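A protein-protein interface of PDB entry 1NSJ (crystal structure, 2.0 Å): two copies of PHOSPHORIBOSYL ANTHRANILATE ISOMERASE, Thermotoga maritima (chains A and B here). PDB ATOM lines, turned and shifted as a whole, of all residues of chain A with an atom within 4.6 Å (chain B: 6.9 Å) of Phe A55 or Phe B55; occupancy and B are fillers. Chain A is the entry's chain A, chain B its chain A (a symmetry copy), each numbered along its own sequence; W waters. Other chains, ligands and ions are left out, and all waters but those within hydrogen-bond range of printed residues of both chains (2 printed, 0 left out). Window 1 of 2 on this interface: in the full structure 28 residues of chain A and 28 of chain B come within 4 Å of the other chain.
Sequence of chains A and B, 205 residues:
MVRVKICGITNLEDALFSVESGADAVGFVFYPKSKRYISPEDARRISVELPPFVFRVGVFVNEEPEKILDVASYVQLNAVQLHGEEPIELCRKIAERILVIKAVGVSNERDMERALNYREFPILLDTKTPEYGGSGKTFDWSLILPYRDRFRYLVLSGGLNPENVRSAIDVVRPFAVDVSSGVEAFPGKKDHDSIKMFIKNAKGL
N of Phe A55 lies within hydrogen-bond range of O of Asp A24 (3.1 Å). The backbone carbonyl oxygen of Val A26 sits at hydrogen-bond distance from the backbone NH of Val A57 (2.9 Å). N of Asn A78 sits at hydrogen-bond distance from O of Arg A56 (2.8 Å). The backbone NH (N) of Ala A79 lies within hydrogen-bond range of the backbone carbonyl oxygen (O) of Arg A56 (3.4 Å). O of Phe B55 sits at hydrogen-bond distance from N of Val B26, at 2.8 Å. The side-chain amide nitrogen (ND2) of Asn B78 sits at hydrogen-bond distance from the backbone carbonyl oxygen (O) of Val B54, 3.5 Å away.
CB of Ala A25 touches CD1 of Phe B53 (3.5 Å). Leu B99 touches Pro A52 (CD2 to CB, 3.8 Å). CB of Pro A52 touches CD1 of Ile B101, at 3.98 Å. CD1 of Phe A53 touches CB of Ala B25, at 3.5 Å. Phe A53 touches Val B57 (CE1 to CG2, 3.9 Å). O of Val A54 touches CE1 of Phe B55, at 3.3 Å. Phe A55 touches Phe B53. Val B54 touches Phe A55 (O to CE1, 3.3 Å). Arg A56 touches Leu B99. Asn B78 touches Asn A78 (OD1 to OD1, 3.8 Å).
Of the printed residues of chain B, Asp A24 touches Asp B24. Of the printed residues of chain B, Val A54 touches Phe B55. Phe A55 touches four residues of chain B. Phe B55 touches four residues of chain A.
Of the 11 printed residues of chain A, 9 touch a printed residue of chain B. Hydrophobic or aromatic side chains of chain A within 4 Å of the printed part of chain B: Ala A25, Pro A52, Phe A53, Phe A55 and Val A57. Of the 21 printed residues of chain B, 9 touch a printed residue of chain A. Among the printed residues, no Asp or Glu carboxylate lies within 4 Å of a Lys or Arg side-chain nitrogen of the other chain.
Asp B24 touches its own counterpart, Asp A24. Val A54 touches Phe B55, and with the chains exchanged Phe A55 touches Val B54. Phe A55 touches its own counterpart, Phe B55. Phe A55 touches Asn B78, and with the chains exchanged Asn A78 touches Phe B55. Of the 16 pairs that touch across the chains among the printed residues, 13 have their exchanged pair printed and touching as well.
Water W2 lies within hydrogen-bond range of O of Asp A24 (2.7 Å), O of Phe B53 (2.8 Å) and N of Phe A55 (3.2 Å). Water W1 lies within hydrogen-bond range of the backbone carbonyl oxygen of Asp B24 (2.7 Å), the backbone carbonyl oxygen of Phe A53 (2.8 Å) and the backbone NH of Phe B55 (3.2 Å).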
ATOM      1  N   ASP A  24     -22.868 -15.307   8.471  1.00  0.00           N
ATOM      2  CA  ASP A  24     -22.540 -16.095   7.289  1.00  0.00           C
ATOM      3  C   ASP A  24     -22.510 -15.294   6.007  1.00  0.00           C
ATOM      4  O   ASP A  24     -22.122 -15.810   4.963  1.00  0.00           O
ATOM      5  CB  ASP A  24     -23.547 -17.235   7.104  1.00  0.00           C
ATOM      6  CG  ASP A  24     -23.747 -18.040   8.365  1.00  0.00           C
ATOM      7  OD1 ASP A  24     -22.984 -18.995   8.592  1.00  0.00           O
ATOM      8  OD2 ASP A  24     -24.679 -17.738   9.130  1.00  0.00           O
ATOM      9  N   ALA A  25     -22.997 -14.061   6.058  1.00  0.00           N
ATOM     10  CA  ALA A  25     -23.041 -13.205   4.878  1.00  0.00           C
ATOM     11  C   ALA A  25     -23.092 -11.758   5.295  1.00  0.00           C
ATOM     12  O   ALA A  25     -23.592 -11.469   6.388  1.00  0.00           O
ATOM     13  CB  ALA A  25     -24.269 -13.544   4.024  1.00  0.00           C
ATOM     14  N   VAL A  26     -22.536 -10.867   4.476  1.00  0.00           N
ATOM     15  CA  VAL A  26     -22.630  -9.435   4.743  1.00  0.00           C
ATOM     16  C   VAL A  26     -23.285  -8.862   3.505  1.00  0.00           C
ATOM     17  O   VAL A  26     -23.093  -9.367   2.378  1.00  0.00           O
ATOM     18  CB  VAL A  26     -21.282  -8.681   4.951  1.00  0.00           C
ATOM     19  CG1 VAL A  26     -20.639  -9.111   6.274  1.00  0.00           C
ATOM     20  CG2 VAL A  26     -20.351  -8.856   3.784  1.00  0.00           C
ATOM     21  N   PRO A  52     -12.605 -16.136   3.255  1.00  0.00           N
ATOM     22  CA  PRO A  52     -13.455 -16.934   2.382  1.00  0.00           C
ATOM     23  C   PRO A  52     -14.550 -17.509   3.292  1.00  0.00           C
ATOM     24  O   PRO A  52     -14.502 -17.335   4.512  1.00  0.00           O
ATOM     25  CB  PRO A  52     -12.507 -18.030   1.904  1.00  0.00           C
ATOM     26  CG  PRO A  52     -11.502 -18.103   3.001  1.00  0.00           C
ATOM     27  CD  PRO A  52     -11.241 -16.675   3.281  1.00  0.00           C
ATOM     28  N   PHE A  53     -15.525 -18.190   2.694  1.00  0.00           N
ATOM     29  CA  PHE A  53     -16.646 -18.810   3.413  1.00  0.00           C
ATOM     30  C   PHE A  53     -17.640 -17.856   4.046  1.00  0.00           C
ATOM     31  O   PHE A  53     -18.317 -18.213   4.995  1.00  0.00           O
ATOM     32  CB  PHE A  53     -16.155 -19.796   4.461  1.00  0.00           C
ATOM     33  CG  PHE A  53     -15.106 -20.700   3.961  1.00  0.00           C
ATOM     34  CD1 PHE A  53     -15.118 -21.108   2.630  1.00  0.00           C
ATOM     35  CD2 PHE A  53     -14.056 -21.084   4.780  1.00  0.00           C
ATOM     36  CE1 PHE A  53     -14.108 -21.904   2.116  1.00  0.00           C
ATOM     37  CE2 PHE A  53     -13.046 -21.879   4.279  1.00  0.00           C
ATOM     38  CZ  PHE A  53     -13.065 -22.283   2.940  1.00  0.00           C
ATOM     39  N   VAL A  54     -17.668 -16.629   3.542  1.00  0.00           N
ATOM     40  CA  VAL A  54     -18.575 -15.592   3.992  1.00  0.00           C
ATOM     41  C   VAL A  54     -19.096 -14.923   2.720  1.00  0.00           C
ATOM     42  O   VAL A  54     -18.318 -14.409   1.918  1.00  0.00           O
ATOM     43  CB  VAL A  54     -17.865 -14.571   4.894  1.00  0.00           C
ATOM     44  CG1 VAL A  54     -18.809 -13.458   5.269  1.00  0.00           C
ATOM     45  CG2 VAL A  54     -17.369 -15.259   6.160  1.00  0.00           C
ATOM     46  N   PHE A  55     -20.410 -15.001   2.507  1.00  0.00           N
ATOM     47  CA  PHE A  55     -21.034 -14.420   1.326  1.00  0.00           C
ATOM     48  C   PHE A  55     -21.061 -12.893   1.313  1.00  0.00           C
ATOM     49  O   PHE A  55     -21.272 -12.257   2.346  1.00  0.00           O
ATOM     50  CB  PHE A  55     -22.466 -14.958   1.180  1.00  0.00           C
ATOM     51  CG  PHE A  55     -22.623 -15.964   0.091  1.00  0.00           C
ATOM     52  CD1 PHE A  55     -21.829 -17.102   0.054  1.00  0.00           C
ATOM     53  CD2 PHE A  55     -23.556 -15.773  -0.909  1.00  0.00           C
ATOM     54  CE1 PHE A  55     -21.967 -18.029  -0.965  1.00  0.00           C
ATOM     55  CE2 PHE A  55     -23.704 -16.700  -1.938  1.00  0.00           C
ATOM     56  CZ  PHE A  55     -22.911 -17.825  -1.965  1.00  0.00           C
ATOM     57  N   ARG A  56     -20.776 -12.314   0.150  1.00  0.00           N
ATOM     58  CA  ARG A  56     -20.842 -10.871  -0.032  1.00  0.00           C
ATOM     59  C   ARG A  56     -22.058 -10.750  -0.928  1.00  0.00           C
ATOM     60  O   ARG A  56     -22.068 -11.302  -2.023  1.00  0.00           O
ATOM     61  CB  ARG A  56     -19.619 -10.328  -0.772  1.00  0.00           C
ATOM     62  CG  ARG A  56     -18.316 -10.373   0.010  1.00  0.00           C
ATOM     63  CD  ARG A  56     -17.493 -11.551  -0.453  1.00  0.00           C
ATOM     64  NE  ARG A  56     -16.079 -11.394  -0.158  1.00  0.00           N
ATOM     65  CZ  ARG A  56     -15.381 -12.225   0.616  1.00  0.00           C
ATOM     66  NH1 ARG A  56     -15.965 -13.270   1.191  1.00  0.00           N
ATOM     67  NH2 ARG A  56     -14.075 -12.043   0.768  1.00  0.00           N
ATOM     68  N   VAL A  57     -23.108 -10.106  -0.444  1.00  0.00           N
ATOM     69  CA  VAL A  57     -24.323  -9.973  -1.234  1.00  0.00           C
ATOM     70  C   VAL A  57     -24.501  -8.513  -1.606  1.00  0.00           C
ATOM     71  O   VAL A  57     -24.190  -7.634  -0.814  1.00  0.00           O
ATOM     72  CB  VAL A  57     -25.548 -10.481  -0.435  1.00  0.00           C
ATOM     73  CG1 VAL A  57     -26.824 -10.336  -1.250  1.00  0.00           C
ATOM     74  CG2 VAL A  57     -25.356 -11.942  -0.044  1.00  0.00           C
ATOM     75  N   ASN A  78     -20.910 -12.558  -4.224  1.00  0.00           N
ATOM     76  CA  ASN A  78     -21.219 -13.985  -4.331  1.00  0.00           C
ATOM     77  C   ASN A  78     -22.690 -14.187  -4.688  1.00  0.00           C
ATOM     78  O   ASN A  78     -23.088 -15.240  -5.192  1.00  0.00           O
ATOM     79  CB  ASN A  78     -20.883 -14.715  -3.023  1.00  0.00           C
ATOM     80  CG  ASN A  78     -19.426 -14.575  -2.646  1.00  0.00           C
ATOM     81  OD1 ASN A  78     -18.549 -14.804  -3.467  1.00  0.00           O
ATOM     82  ND2 ASN A  78     -19.163 -14.174  -1.420  1.00  0.00           N
ATOM     83  N   ALA A  79     -23.491 -13.152  -4.462  1.00  0.00           N
ATOM     84  CA  ALA A  79     -24.912 -13.209  -4.759  1.00  0.00           C
ATOM     85  C   ALA A  79     -25.441 -11.807  -4.924  1.00  0.00           C
ATOM     86  O   ALA A  79     -24.856 -10.828  -4.420  1.00  0.00           O
ATOM     87  CB  ALA A  79     -25.680 -13.925  -3.639  1.00  0.00           C
ATOM     88  N   LYS B   5     -15.316 -26.702   5.762  1.00  0.00           N
ATOM     89  CA  LYS B   5     -15.477 -26.982   4.341  1.00  0.00           C
ATOM     90  C   LYS B   5     -15.409 -28.510   4.166  1.00  0.00           C
ATOM     91  O   LYS B   5     -14.552 -29.161   4.771  1.00  0.00           O
ATOM     92  CB  LYS B   5     -14.371 -26.292   3.530  1.00  0.00           C
ATOM     93  CG  LYS B   5     -14.188 -26.833   2.107  1.00  0.00           C
ATOM     94  CD  LYS B   5     -13.220 -25.986   1.279  1.00  0.00           C
ATOM     95  CE  LYS B   5     -12.832 -26.662  -0.040  1.00  0.00           C
ATOM     96  NZ  LYS B   5     -11.888 -27.811   0.128  1.00  0.00           N
ATOM     97  N   ALA B  23     -22.244 -27.326   7.266  1.00  0.00           N
ATOM     98  CA  ALA B  23     -21.018 -27.007   6.542  1.00  0.00           C
ATOM     99  C   ALA B  23     -21.141 -25.627   5.905  1.00  0.00           C
ATOM    100  O   ALA B  23     -22.194 -25.277   5.395  1.00  0.00           O
ATOM    101  CB  ALA B  23     -20.757 -28.042   5.491  1.00  0.00           C
ATOM    102  N   ASP B  24     -20.059 -24.855   5.906  1.00  0.00           N
ATOM    103  CA  ASP B  24     -20.055 -23.504   5.357  1.00  0.00           C
ATOM    104  C   ASP B  24     -19.566 -23.426   3.929  1.00  0.00           C
ATOM    105  O   ASP B  24     -19.636 -22.368   3.308  1.00  0.00           O
ATOM    106  CB  ASP B  24     -19.175 -22.579   6.205  1.00  0.00           C
ATOM    107  CG  ASP B  24     -19.499 -22.663   7.676  1.00  0.00           C
ATOM    108  OD1 ASP B  24     -20.393 -21.930   8.135  1.00  0.00           O
ATOM    109  OD2 ASP B  24     -18.849 -23.445   8.391  1.00  0.00           O
ATOM    110  N   ALA B  25     -18.994 -24.513   3.429  1.00  0.00           N
ATOM    111  CA  ALA B  25     -18.464 -24.544   2.070  1.00  0.00           C
ATOM    112  C   ALA B  25     -18.398 -25.966   1.578  1.00  0.00           C
ATOM    113  O   ALA B  25     -18.265 -26.877   2.401  1.00  0.00           O
ATOM    114  CB  ALA B  25     -17.064 -23.915   2.033  1.00  0.00           C
ATOM    115  N   VAL B  26     -18.547 -26.165   0.269  1.00  0.00           N
ATOM    116  CA  VAL B  26     -18.392 -27.495  -0.313  1.00  0.00           C
ATOM    117  C   VAL B  26     -17.302 -27.329  -1.350  1.00  0.00           C
ATOM    118  O   VAL B  26     -17.159 -26.256  -1.973  1.00  0.00           O
ATOM    119  CB  VAL B  26     -19.642 -28.081  -1.038  1.00  0.00           C
ATOM    120  CG1 VAL B  26     -20.734 -28.413  -0.015  1.00  0.00           C
ATOM    121  CG2 VAL B  26     -20.141 -27.173  -2.127  1.00  0.00           C
ATOM    122  N   GLY B  27     -16.497 -28.373  -1.530  1.00  0.00           N
ATOM    123  CA  GLY B  27     -15.433 -28.328  -2.498  1.00  0.00           C
ATOM    124  C   GLY B  27     -15.582 -29.355  -3.621  1.00  0.00           C
ATOM    125  O   GLY B  27     -15.945 -30.490  -3.347  1.00  0.00           O
ATOM    126  N   PHE B  28     -15.308 -28.932  -4.851  1.00  0.00           N
ATOM    127  CA  PHE B  28     -15.354 -29.761  -6.070  1.00  0.00           C
ATOM    128  C   PHE B  28     -13.920 -29.844  -6.594  1.00  0.00           C
ATOM    129  O   PHE B  28     -13.283 -28.817  -6.807  1.00  0.00           O
ATOM    130  CB  PHE B  28     -16.222 -29.117  -7.160  1.00  0.00           C
ATOM    131  CG  PHE B  28     -17.645 -28.841  -6.733  1.00  0.00           C
ATOM    132  CD1 PHE B  28     -18.499 -29.887  -6.392  1.00  0.00           C
ATOM    133  CD2 PHE B  28     -18.127 -27.529  -6.680  1.00  0.00           C
ATOM    134  CE1 PHE B  28     -19.804 -29.632  -6.001  1.00  0.00           C
ATOM    135  CE2 PHE B  28     -19.420 -27.267  -6.292  1.00  0.00           C
ATOM    136  CZ  PHE B  28     -20.262 -28.319  -5.952  1.00  0.00           C
ATOM    137  N   LEU B  50     -27.741 -25.629  -4.774  1.00  0.00           N
ATOM    138  CA  LEU B  50     -27.376 -25.282  -3.401  1.00  0.00           C
ATOM    139  C   LEU B  50     -27.902 -23.917  -2.987  1.00  0.00           C
ATOM    140  O   LEU B  50     -28.058 -23.037  -3.815  1.00  0.00           O
ATOM    141  CB  LEU B  50     -25.849 -25.306  -3.252  1.00  0.00           C
ATOM    142  CG  LEU B  50     -25.136 -26.648  -3.446  1.00  0.00           C
ATOM    143  CD1 LEU B  50     -23.619 -26.465  -3.334  1.00  0.00           C
ATOM    144  CD2 LEU B  50     -25.633 -27.639  -2.412  1.00  0.00           C
ATOM    145  N   PRO B  51     -28.157 -23.720  -1.686  1.00  0.00           N
ATOM    146  CA  PRO B  51     -28.660 -22.432  -1.208  1.00  0.00           C
ATOM    147  C   PRO B  51     -27.587 -21.355  -1.158  1.00  0.00           C
ATOM    148  O   PRO B  51     -26.396 -21.624  -1.357  1.00  0.00           O
ATOM    149  CB  PRO B  51     -29.077 -22.766   0.216  1.00  0.00           C
ATOM    150  CG  PRO B  51     -28.052 -23.777   0.616  1.00  0.00           C
ATOM    151  CD  PRO B  51     -28.040 -24.676  -0.579  1.00  0.00           C
ATOM    152  N   PRO B  52     -28.004 -20.094  -0.980  1.00  0.00           N
ATOM    153  CA  PRO B  52     -27.004 -19.040  -0.896  1.00  0.00           C
ATOM    154  C   PRO B  52     -26.347 -19.208   0.482  1.00  0.00           C
ATOM    155  O   PRO B  52     -26.781 -20.039   1.283  1.00  0.00           O
ATOM    156  CB  PRO B  52     -27.850 -17.771  -0.950  1.00  0.00           C
ATOM    157  CG  PRO B  52     -29.166 -18.226  -0.421  1.00  0.00           C
ATOM    158  CD  PRO B  52     -29.349 -19.521  -1.111  1.00  0.00           C
ATOM    159  N   PHE B  53     -25.308 -18.419   0.747  1.00  0.00           N
ATOM    160  CA  PHE B  53     -24.567 -18.444   2.015  1.00  0.00           C
ATOM    161  C   PHE B  53     -23.745 -19.690   2.281  1.00  0.00           C
ATOM    162  O   PHE B  53     -23.469 -20.013   3.424  1.00  0.00           O
ATOM    163  CB  PHE B  53     -25.485 -18.184   3.198  1.00  0.00           C
ATOM    164  CG  PHE B  53     -26.398 -17.048   2.985  1.00  0.00           C
ATOM    165  CD1 PHE B  53     -25.985 -15.959   2.222  1.00  0.00           C
ATOM    166  CD2 PHE B  53     -27.697 -17.086   3.467  1.00  0.00           C
ATOM    167  CE1 PHE B  53     -26.844 -14.908   1.950  1.00  0.00           C
ATOM    168  CE2 PHE B  53     -28.561 -16.043   3.204  1.00  0.00           C
ATOM    169  CZ  PHE B  53     -28.138 -14.955   2.435  1.00  0.00           C
ATOM    170  N   VAL B  54     -23.417 -20.407   1.214  1.00  0.00           N
ATOM    171  CA  VAL B  54     -22.606 -21.607   1.266  1.00  0.00           C
ATOM    172  C   VAL B  54     -21.619 -21.486   0.105  1.00  0.00           C
ATOM    173  O   VAL B  54     -22.022 -21.364  -1.051  1.00  0.00           O
ATOM    174  CB  VAL B  54     -23.462 -22.875   1.124  1.00  0.00           C
ATOM    175  CG1 VAL B  54     -22.583 -24.098   1.089  1.00  0.00           C
ATOM    176  CG2 VAL B  54     -24.425 -22.981   2.300  1.00  0.00           C
ATOM    177  N   PHE B  55     -20.327 -21.444   0.430  1.00  0.00           N
ATOM    178  CA  PHE B  55     -19.283 -21.314  -0.578  1.00  0.00           C
ATOM    179  C   PHE B  55     -19.087 -22.554  -1.448  1.00  0.00           C
ATOM    180  O   PHE B  55     -19.167 -23.683  -0.963  1.00  0.00           O
ATOM    181  CB  PHE B  55     -17.953 -20.948   0.098  1.00  0.00           C
ATOM    182  CG  PHE B  55     -17.551 -19.526  -0.095  1.00  0.00           C
ATOM    183  CD1 PHE B  55     -18.405 -18.490   0.258  1.00  0.00           C
ATOM    184  CD2 PHE B  55     -16.321 -19.214  -0.641  1.00  0.00           C
ATOM    185  CE1 PHE B  55     -18.035 -17.170   0.067  1.00  0.00           C
ATOM    186  CE2 PHE B  55     -15.939 -17.889  -0.838  1.00  0.00           C
ATOM    187  CZ  PHE B  55     -16.795 -16.870  -0.484  1.00  0.00           C
ATOM    188  N   ARG B  56     -18.901 -22.334  -2.746  1.00  0.00           N
ATOM    189  CA  ARG B  56     -18.621 -23.414  -3.682  1.00  0.00           C
ATOM    190  C   ARG B  56     -17.169 -23.135  -4.015  1.00  0.00           C
ATOM    191  O   ARG B  56     -16.853 -22.063  -4.521  1.00  0.00           O
ATOM    192  CB  ARG B  56     -19.458 -23.302  -4.957  1.00  0.00           C
ATOM    193  CG  ARG B  56     -20.945 -23.568  -4.781  1.00  0.00           C
ATOM    194  CD  ARG B  56     -21.688 -22.255  -4.734  1.00  0.00           C
ATOM    195  NE  ARG B  56     -23.093 -22.397  -5.075  1.00  0.00           N
ATOM    196  CZ  ARG B  56     -24.096 -22.084  -4.256  1.00  0.00           C
ATOM    197  NH1 ARG B  56     -23.856 -21.622  -3.033  1.00  0.00           N
ATOM    198  NH2 ARG B  56     -25.349 -22.176  -4.683  1.00  0.00           N
ATOM    199  N   VAL B  57     -16.279 -24.049  -3.666  1.00  0.00           N
ATOM    200  CA  VAL B  57     -14.863 -23.841  -3.928  1.00  0.00           C
ATOM    201  C   VAL B  57     -14.413 -24.839  -4.978  1.00  0.00           C
ATOM    202  O   VAL B  57     -14.873 -25.972  -4.988  1.00  0.00           O
ATOM    203  CB  VAL B  57     -14.039 -24.014  -2.629  1.00  0.00           C
ATOM    204  CG1 VAL B  57     -12.556 -23.808  -2.895  1.00  0.00           C
ATOM    205  CG2 VAL B  57     -14.509 -23.025  -1.568  1.00  0.00           C
ATOM    206  N   LEU B  77     -18.457 -20.679  -9.070  1.00  0.00           N
ATOM    207  CA  LEU B  77     -17.664 -20.910  -7.875  1.00  0.00           C
ATOM    208  C   LEU B  77     -17.542 -19.593  -7.156  1.00  0.00           C
ATOM    209  O   LEU B  77     -17.639 -18.544  -7.775  1.00  0.00           O
ATOM    210  CB  LEU B  77     -16.260 -21.408  -8.251  1.00  0.00           C
ATOM    211  CG  LEU B  77     -16.175 -22.823  -8.830  1.00  0.00           C
ATOM    212  CD1 LEU B  77     -14.730 -23.150  -9.165  1.00  0.00           C
ATOM    213  CD2 LEU B  77     -16.730 -23.824  -7.843  1.00  0.00           C
ATOM    214  N   ASN B  78     -17.336 -19.661  -5.847  1.00  0.00           N
ATOM    215  CA  ASN B  78     -17.167 -18.470  -5.012  1.00  0.00           C
ATOM    216  C   ASN B  78     -15.692 -18.263  -4.673  1.00  0.00           C
ATOM    217  O   ASN B  78     -15.266 -17.161  -4.319  1.00  0.00           O
ATOM    218  CB  ASN B  78     -17.999 -18.583  -3.728  1.00  0.00           C
ATOM    219  CG  ASN B  78     -19.473 -18.753  -4.013  1.00  0.00           C
ATOM    220  OD1 ASN B  78     -20.044 -18.003  -4.793  1.00  0.00           O
ATOM    221  ND2 ASN B  78     -20.087 -19.748  -3.408  1.00  0.00           N
ATOM    222  N   ALA B  79     -14.905 -19.323  -4.823  1.00  0.00           N
ATOM    223  CA  ALA B  79     -13.483 -19.262  -4.537  1.00  0.00           C
ATOM    224  C   ALA B  79     -12.779 -20.369  -5.281  1.00  0.00           C
ATOM    225  O   ALA B  79     -13.389 -21.389  -5.656  1.00  0.00           O
ATOM    226  CB  ALA B  79     -13.217 -19.399  -3.031  1.00  0.00           C
ATOM    227  N   VAL B  80     -11.489 -20.149  -5.509  1.00  0.00           N
ATOM    228  CA  VAL B  80     -10.633 -21.102  -6.192  1.00  0.00           C
ATOM    229  C   VAL B  80      -9.538 -21.516  -5.180  1.00  0.00           C
ATOM    230  O   VAL B  80      -9.032 -20.684  -4.440  1.00  0.00           O
ATOM    231  CB  VAL B  80     -10.065 -20.434  -7.476  1.00  0.00           C
ATOM    232  CG1 VAL B  80      -8.753 -21.003  -7.877  1.00  0.00           C
ATOM    233  CG2 VAL B  80     -11.048 -20.611  -8.591  1.00  0.00           C
ATOM    234  N   LEU B  99     -11.865 -14.833  -5.519  1.00  0.00           N
ATOM    235  CA  LEU B  99     -11.065 -15.107  -4.322  1.00  0.00           C
ATOM    236  C   LEU B  99     -10.225 -16.413  -4.436  1.00  0.00           C
ATOM    237  O   LEU B  99     -10.727 -17.470  -4.890  1.00  0.00           O
ATOM    238  CB  LEU B  99     -11.995 -15.159  -3.098  1.00  0.00           C
ATOM    239  CG  LEU B  99     -11.469 -15.207  -1.664  1.00  0.00           C
ATOM    240  CD1 LEU B  99     -12.544 -14.727  -0.739  1.00  0.00           C
ATOM    241  CD2 LEU B  99     -11.054 -16.607  -1.282  1.00  0.00           C
ATOM    242  N   ILE B 101      -7.565 -19.267  -2.517  1.00  0.00           N
ATOM    243  CA  ILE B 101      -7.042 -19.873  -1.310  1.00  0.00           C
ATOM    244  C   ILE B 101      -5.837 -20.681  -1.832  1.00  0.00           C
ATOM    245  O   ILE B 101      -5.972 -21.456  -2.795  1.00  0.00           O
ATOM    246  CB  ILE B 101      -8.063 -20.837  -0.687  1.00  0.00           C
ATOM    247  CG1 ILE B 101      -9.295 -20.057  -0.238  1.00  0.00           C
ATOM    248  CG2 ILE B 101      -7.449 -21.591   0.484  1.00  0.00           C
ATOM    249  CD1 ILE B 101     -10.467 -20.950   0.137  1.00  0.00           C
HETATM  250  O   HOH W   1     -19.735 -19.729   3.067  1.00  0.00           O
HETATM  251  O   HOH W   2     -21.660 -17.835   3.314  1.00  0.00           O
